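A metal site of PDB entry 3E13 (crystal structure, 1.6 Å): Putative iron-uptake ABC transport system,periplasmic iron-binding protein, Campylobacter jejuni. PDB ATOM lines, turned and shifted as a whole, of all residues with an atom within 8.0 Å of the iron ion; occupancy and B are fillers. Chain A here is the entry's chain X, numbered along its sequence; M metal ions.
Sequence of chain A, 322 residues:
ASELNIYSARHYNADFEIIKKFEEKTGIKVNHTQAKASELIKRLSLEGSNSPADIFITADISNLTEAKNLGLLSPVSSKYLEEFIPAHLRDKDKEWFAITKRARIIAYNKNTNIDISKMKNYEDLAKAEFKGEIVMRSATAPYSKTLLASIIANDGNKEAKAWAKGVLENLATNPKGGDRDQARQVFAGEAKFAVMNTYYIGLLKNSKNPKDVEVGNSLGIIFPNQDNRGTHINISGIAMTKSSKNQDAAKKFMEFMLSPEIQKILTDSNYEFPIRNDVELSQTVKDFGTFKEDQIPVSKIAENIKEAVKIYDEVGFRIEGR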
ATOM      1  N   ALA A   9      36.723   3.675   9.593  1.00  0.00           N
ATOM      2  CA  ALA A   9      35.624   2.924  10.158  1.00  0.00           C
ATOM      3  C   ALA A   9      34.761   3.776  11.095  1.00  0.00           C
ATOM      4  O   ALA A   9      33.882   3.271  11.740  1.00  0.00           O
ATOM      5  CB  ALA A   9      36.130   1.651  10.865  1.00  0.00           C
ATOM      6  N   ARG A  10      35.049   5.078  11.149  1.00  0.00           N
ATOM      7  CA  ARG A  10      34.104   6.030  11.734  1.00  0.00           C
ATOM      8  C   ARG A  10      32.858   6.110  10.815  1.00  0.00           C
ATOM      9  O   ARG A  10      32.849   5.560   9.701  1.00  0.00           O
ATOM     10  CB  ARG A  10      34.769   7.388  11.971  1.00  0.00           C
ATOM     11  CG  ARG A  10      35.644   7.378  13.193  1.00  0.00           C
ATOM     12  CD  ARG A  10      36.376   8.679  13.445  1.00  0.00           C
ATOM     13  NE  ARG A  10      35.504   9.833  13.624  1.00  0.00           N
ATOM     14  CZ  ARG A  10      35.034  10.279  14.846  1.00  0.00           C
ATOM     15  NH1 ARG A  10      35.346   9.661  15.995  1.00  0.00           N
ATOM     16  NH2 ARG A  10      34.280  11.379  14.884  1.00  0.00           N
ATOM     17  N   HIS A  11      31.785   6.725  11.294  1.00  0.00           N
ATOM     18  CA  HIS A  11      30.510   6.667  10.602  1.00  0.00           C
ATOM     19  C   HIS A  11      29.648   7.862  10.996  1.00  0.00           C
ATOM     20  O   HIS A  11      28.486   7.708  11.416  1.00  0.00           O
ATOM     21  CB  HIS A  11      29.844   5.308  10.933  1.00  0.00           C
ATOM     22  CG  HIS A  11      30.083   4.865  12.352  1.00  0.00           C
ATOM     23  ND1 HIS A  11      31.129   4.043  12.715  1.00  0.00           N
ATOM     24  CD2 HIS A  11      29.431   5.176  13.514  1.00  0.00           C
ATOM     25  CE1 HIS A  11      31.105   3.860  14.036  1.00  0.00           C
ATOM     26  NE2 HIS A  11      30.072   4.521  14.536  1.00  0.00           N
ATOM     27  N   TYR A  12      30.259   9.054  10.853  1.00  0.00           N
ATOM     28  CA  TYR A  12      29.686  10.291  11.373  1.00  0.00           C
ATOM     29  C   TYR A  12      29.723  11.412  10.358  1.00  0.00           C
ATOM     30  O   TYR A  12      30.714  11.629   9.667  1.00  0.00           O
ATOM     31  CB  TYR A  12      30.482  10.736  12.599  1.00  0.00           C
ATOM     32  CG  TYR A  12      30.655   9.644  13.629  1.00  0.00           C
ATOM     33  CD1 TYR A  12      31.928   9.118  13.895  1.00  0.00           C
ATOM     34  CD2 TYR A  12      29.583   9.050  14.242  1.00  0.00           C
ATOM     35  CE1 TYR A  12      32.124   8.102  14.791  1.00  0.00           C
ATOM     36  CE2 TYR A  12      29.769   8.026  15.133  1.00  0.00           C
ATOM     37  CZ  TYR A  12      31.019   7.557  15.432  1.00  0.00           C
ATOM     38  OH  TYR A  12      31.106   6.518  16.336  1.00  0.00           O
ATOM     39  N   ALA A  59      36.788   3.614  15.250  1.00  0.00           N
ATOM     40  CA  ALA A  59      35.989   4.032  16.365  1.00  0.00           C
ATOM     41  C   ALA A  59      36.192   3.050  17.535  1.00  0.00           C
ATOM     42  O   ALA A  59      35.300   2.806  18.343  1.00  0.00           O
ATOM     43  CB  ALA A  59      34.521   4.082  15.922  1.00  0.00           C
ATOM     44  N   ASP A  60      37.385   2.478  17.600  1.00  0.00           N
ATOM     45  CA  ASP A  60      37.654   1.364  18.505  1.00  0.00           C
ATOM     46  C   ASP A  60      39.131   1.120  18.703  1.00  0.00           C
ATOM     47  O   ASP A  60      39.928   1.066  17.739  1.00  0.00           O
ATOM     48  CB  ASP A  60      36.991   0.106  17.957  1.00  0.00           C
ATOM     49  CG  ASP A  60      37.312  -1.099  18.722  1.00  0.00           C
ATOM     50  OD1 ASP A  60      37.882  -2.091  18.125  1.00  0.00           O
ATOM     51  OD2 ASP A  60      36.989  -1.198  19.929  1.00  0.00           O
ATOM     52  N   ARG A 102      34.953   7.698  24.377  1.00  0.00           N
ATOM     53  CA  ARG A 102      33.500   7.437  24.475  1.00  0.00           C
ATOM     54  C   ARG A 102      33.259   6.374  25.545  1.00  0.00           C
ATOM     55  O   ARG A 102      34.119   5.617  25.848  1.00  0.00           O
ATOM     56  CB  ARG A 102      32.940   7.031  23.095  1.00  0.00           C
ATOM     57  CG  ARG A 102      33.671   5.838  22.452  1.00  0.00           C
ATOM     58  CD  ARG A 102      34.768   6.245  21.427  1.00  0.00           C
ATOM     59  NE  ARG A 102      34.223   6.983  20.310  1.00  0.00           N
ATOM     60  CZ  ARG A 102      33.465   6.510  19.314  1.00  0.00           C
ATOM     61  NH1 ARG A 102      33.132   5.237  19.267  1.00  0.00           N
ATOM     62  NH2 ARG A 102      33.075   7.299  18.332  1.00  0.00           N
ATOM     63  N   ARG A 104      30.695   3.220  26.995  1.00  0.00           N
ATOM     64  CA  ARG A 104      29.645   2.295  26.634  1.00  0.00           C
ATOM     65  C   ARG A 104      28.812   2.078  27.899  1.00  0.00           C
ATOM     66  O   ARG A 104      29.257   1.469  28.892  1.00  0.00           O
ATOM     67  CB  ARG A 104      30.223   1.000  26.058  1.00  0.00           C
ATOM     68  CG  ARG A 104      29.165   0.187  25.323  1.00  0.00           C
ATOM     69  CD  ARG A 104      29.743  -0.610  24.229  1.00  0.00           C
ATOM     70  NE  ARG A 104      28.740  -1.227  23.360  1.00  0.00           N
ATOM     71  CZ  ARG A 104      28.066  -0.597  22.390  1.00  0.00           C
ATOM     72  NH1 ARG A 104      28.258   0.683  22.198  1.00  0.00           N
ATOM     73  NH2 ARG A 104      27.161  -1.227  21.639  1.00  0.00           N
ATOM     74  N   ARG A 137      23.581  -4.608  20.054  1.00  0.00           N
ATOM     75  CA  ARG A 137      23.949  -4.914  18.672  1.00  0.00           C
ATOM     76  C   ARG A 137      24.805  -6.170  18.557  1.00  0.00           C
ATOM     77  O   ARG A 137      25.230  -6.789  19.548  1.00  0.00           O
ATOM     78  CB  ARG A 137      24.684  -3.746  18.086  1.00  0.00           C
ATOM     79  CG  ARG A 137      26.093  -3.549  18.550  1.00  0.00           C
ATOM     80  CD  ARG A 137      26.684  -2.270  18.125  1.00  0.00           C
ATOM     81  NE  ARG A 137      26.764  -2.129  16.673  1.00  0.00           N
ATOM     82  CZ  ARG A 137      26.973  -0.989  16.031  1.00  0.00           C
ATOM     83  NH1 ARG A 137      27.092   0.177  16.685  1.00  0.00           N
ATOM     84  NH2 ARG A 137      27.052  -0.972  14.726  1.00  0.00           N
ATOM     85  N   TYR A 143      32.373  -2.331  19.062  1.00  0.00           N
ATOM     86  CA  TYR A 143      32.002  -1.940  20.451  1.00  0.00           C
ATOM     87  C   TYR A 143      31.686  -3.156  21.303  1.00  0.00           C
ATOM     88  O   TYR A 143      32.087  -3.207  22.460  1.00  0.00           O
ATOM     89  CB  TYR A 143      30.840  -0.976  20.523  1.00  0.00           C
ATOM     90  CG  TYR A 143      30.957   0.200  19.570  1.00  0.00           C
ATOM     91  CD1 TYR A 143      32.182   0.792  19.245  1.00  0.00           C
ATOM     92  CD2 TYR A 143      29.823   0.764  19.030  1.00  0.00           C
ATOM     93  CE1 TYR A 143      32.237   1.815  18.351  1.00  0.00           C
ATOM     94  CE2 TYR A 143      29.878   1.841  18.170  1.00  0.00           C
ATOM     95  CZ  TYR A 143      31.105   2.395  17.863  1.00  0.00           C
ATOM     96  OH  TYR A 143      31.215   3.382  16.914  1.00  0.00           O
ATOM     97  N   ASP A 179      23.712   0.972  17.650  1.00  0.00           N
ATOM     98  CA  ASP A 179      23.346   1.657  18.867  1.00  0.00           C
ATOM     99  C   ASP A 179      22.078   2.515  18.792  1.00  0.00           C
ATOM    100  O   ASP A 179      21.281   2.508  19.715  1.00  0.00           O
ATOM    101  CB  ASP A 179      24.509   2.530  19.339  1.00  0.00           C
ATOM    102  CG  ASP A 179      25.680   1.752  19.912  1.00  0.00           C
ATOM    103  OD1 ASP A 179      26.039   0.659  19.361  1.00  0.00           O
ATOM    104  OD2 ASP A 179      26.417   2.216  20.825  1.00  0.00           O
ATOM    105  N   ARG A 180      21.933   3.334  17.727  1.00  0.00           N
ATOM    106  CA  ARG A 180      20.771   4.197  17.622  1.00  0.00           C
ATOM    107  C   ARG A 180      19.482   3.392  17.464  1.00  0.00           C
ATOM    108  O   ARG A 180      18.390   3.836  17.840  1.00  0.00           O
ATOM    109  CB  ARG A 180      20.946   5.186  16.492  1.00  0.00           C
ATOM    110  CG  ARG A 180      21.986   6.240  16.784  1.00  0.00           C
ATOM    111  CD  ARG A 180      22.281   7.095  15.661  1.00  0.00           C
ATOM    112  NE  ARG A 180      23.242   6.402  14.840  1.00  0.00           N
ATOM    113  CZ  ARG A 180      24.076   6.967  13.991  1.00  0.00           C
ATOM    114  NH1 ARG A 180      24.094   8.275  13.836  1.00  0.00           N
ATOM    115  NH2 ARG A 180      24.918   6.181  13.331  1.00  0.00           N
ATOM    116  N   ASN A 197      26.773   3.610  23.249  1.00  0.00           N
ATOM    117  CA  ASN A 197      27.783   4.627  23.524  1.00  0.00           C
ATOM    118  C   ASN A 197      27.115   5.971  23.806  1.00  0.00           C
ATOM    119  O   ASN A 197      26.028   6.322  23.296  1.00  0.00           O
ATOM    120  CB  ASN A 197      28.760   4.801  22.370  1.00  0.00           C
ATOM    121  CG  ASN A 197      29.727   3.647  22.193  1.00  0.00           C
ATOM    122  OD1 ASN A 197      29.980   2.845  23.125  1.00  0.00           O
ATOM    123  ND2 ASN A 197      30.297   3.552  20.989  1.00  0.00           N
ATOM    124  N   TYR A 199      27.857   9.129  23.118  1.00  0.00           N
ATOM    125  CA  TYR A 199      27.746  10.165  22.088  1.00  0.00           C
ATOM    126  C   TYR A 199      26.487  10.018  21.245  1.00  0.00           C
ATOM    127  O   TYR A 199      25.952  10.973  20.760  1.00  0.00           O
ATOM    128  CB  TYR A 199      29.012  10.284  21.222  1.00  0.00           C
ATOM    129  CG  TYR A 199      29.377   9.027  20.548  1.00  0.00           C
ATOM    130  CD1 TYR A 199      28.853   8.740  19.299  1.00  0.00           C
ATOM    131  CD2 TYR A 199      30.198   8.092  21.166  1.00  0.00           C
ATOM    132  CE1 TYR A 199      29.112   7.544  18.703  1.00  0.00           C
ATOM    133  CE2 TYR A 199      30.476   6.893  20.557  1.00  0.00           C
ATOM    134  CZ  TYR A 199      29.955   6.625  19.331  1.00  0.00           C
ATOM    135  OH  TYR A 199      30.198   5.409  18.702  1.00  0.00           O
ATOM    136  N   TYR A 200      26.009   8.774  21.073  1.00  0.00           N
ATOM    137  CA  TYR A 200      24.772   8.609  20.296  1.00  0.00           C
ATOM    138  C   TYR A 200      23.590   9.301  20.960  1.00  0.00           C
ATOM    139  O   TYR A 200      22.700   9.776  20.254  1.00  0.00           O
ATOM    140  CB  TYR A 200      24.398   7.126  20.077  1.00  0.00           C
ATOM    141  CG  TYR A 200      25.386   6.437  19.130  1.00  0.00           C
ATOM    142  CD1 TYR A 200      25.481   6.830  17.818  1.00  0.00           C
ATOM    143  CD2 TYR A 200      26.190   5.376  19.567  1.00  0.00           C
ATOM    144  CE1 TYR A 200      26.381   6.221  16.947  1.00  0.00           C
ATOM    145  CE2 TYR A 200      27.095   4.799  18.734  1.00  0.00           C
ATOM    146  CZ  TYR A 200      27.203   5.193  17.433  1.00  0.00           C
ATOM    147  OH  TYR A 200      28.076   4.635  16.573  1.00  0.00           O
ATOM    148  N   LEU A 203      23.918  12.789  19.750  1.00  0.00           N
ATOM    149  CA  LEU A 203      23.625  12.913  18.346  1.00  0.00           C
ATOM    150  C   LEU A 203      22.110  12.900  18.148  1.00  0.00           C
ATOM    151  O   LEU A 203      21.577  13.667  17.360  1.00  0.00           O
ATOM    152  CB  LEU A 203      24.260  11.768  17.542  1.00  0.00           C
ATOM    153  CG  LEU A 203      25.736  11.940  17.240  1.00  0.00           C
ATOM    154  CD1 LEU A 203      26.344  10.663  16.671  1.00  0.00           C
ATOM    155  CD2 LEU A 203      25.976  13.079  16.330  1.00  0.00           C
ATOM    156  N   SER A 236      38.058   6.418  19.805  1.00  0.00           N
ATOM    157  CA  SER A 236      38.203   6.472  18.380  1.00  0.00           C
ATOM    158  C   SER A 236      39.675   6.900  18.230  1.00  0.00           C
ATOM    159  O   SER A 236      40.240   7.652  19.051  1.00  0.00           O
ATOM    160  CB  SER A 236      37.259   7.478  17.744  1.00  0.00           C
ATOM    161  OG  SER A 236      37.588   7.757  16.407  1.00  0.00           O
ATOM    162  N   ASN A 270      29.760  16.051  17.473  1.00  0.00           N
ATOM    163  CA  ASN A 270      29.648  14.592  17.571  1.00  0.00           C
ATOM    164  C   ASN A 270      29.445  14.044  18.962  1.00  0.00           C
ATOM    165  O   ASN A 270      29.269  12.843  19.111  1.00  0.00           O
ATOM    166  CB  ASN A 270      30.812  13.866  16.859  1.00  0.00           C
ATOM    167  CG  ASN A 270      30.340  12.586  16.187  1.00  0.00           C
ATOM    168  OD1 ASN A 270      29.342  12.610  15.444  1.00  0.00           O
ATOM    169  ND2 ASN A 270      31.033  11.478  16.454  1.00  0.00           N
ATOM    170  N   GLU A 272      31.264  13.496  21.504  1.00  0.00           N
ATOM    171  CA  GLU A 272      32.292  12.639  22.083  1.00  0.00           C
ATOM    172  C   GLU A 272      33.053  13.409  23.128  1.00  0.00           C
ATOM    173  O   GLU A 272      32.886  14.626  23.271  1.00  0.00           O
ATOM    174  CB  GLU A 272      33.231  12.107  21.022  1.00  0.00           C
ATOM    175  CG  GLU A 272      32.544  11.243  19.956  1.00  0.00           C
ATOM    176  CD  GLU A 272      33.464  10.838  18.828  1.00  0.00           C
ATOM    177  OE1 GLU A 272      33.499  11.562  17.822  1.00  0.00           O
ATOM    178  OE2 GLU A 272      34.132   9.798  18.974  1.00  0.00           O
HETATM  179 FE    FE M   1      30.000   4.948  16.690  1.00  0.00          FE
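A ring nitrogen (ND1) of His 11 sits at hydrogen-bond distance from the backbone carbonyl oxygen of Ala 9, 3.0 Å away. The side-chain amide nitrogen of Asn 197 lies close to the side-chain hydroxyl of Tyr 199. The guanidinium group of Arg 102 lies close to the side-chain hydroxyl of Tyr 199, 3.0 Å away. The side-chain hydroxyl of Tyr 12 sits close to the guanidinium group of Arg 102 (2.9 Å).
The iron ion is bound by OH of Tyr 200, OH of Tyr 12, OH of Tyr 143, OH of Tyr 199 and NE2 of His 11.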
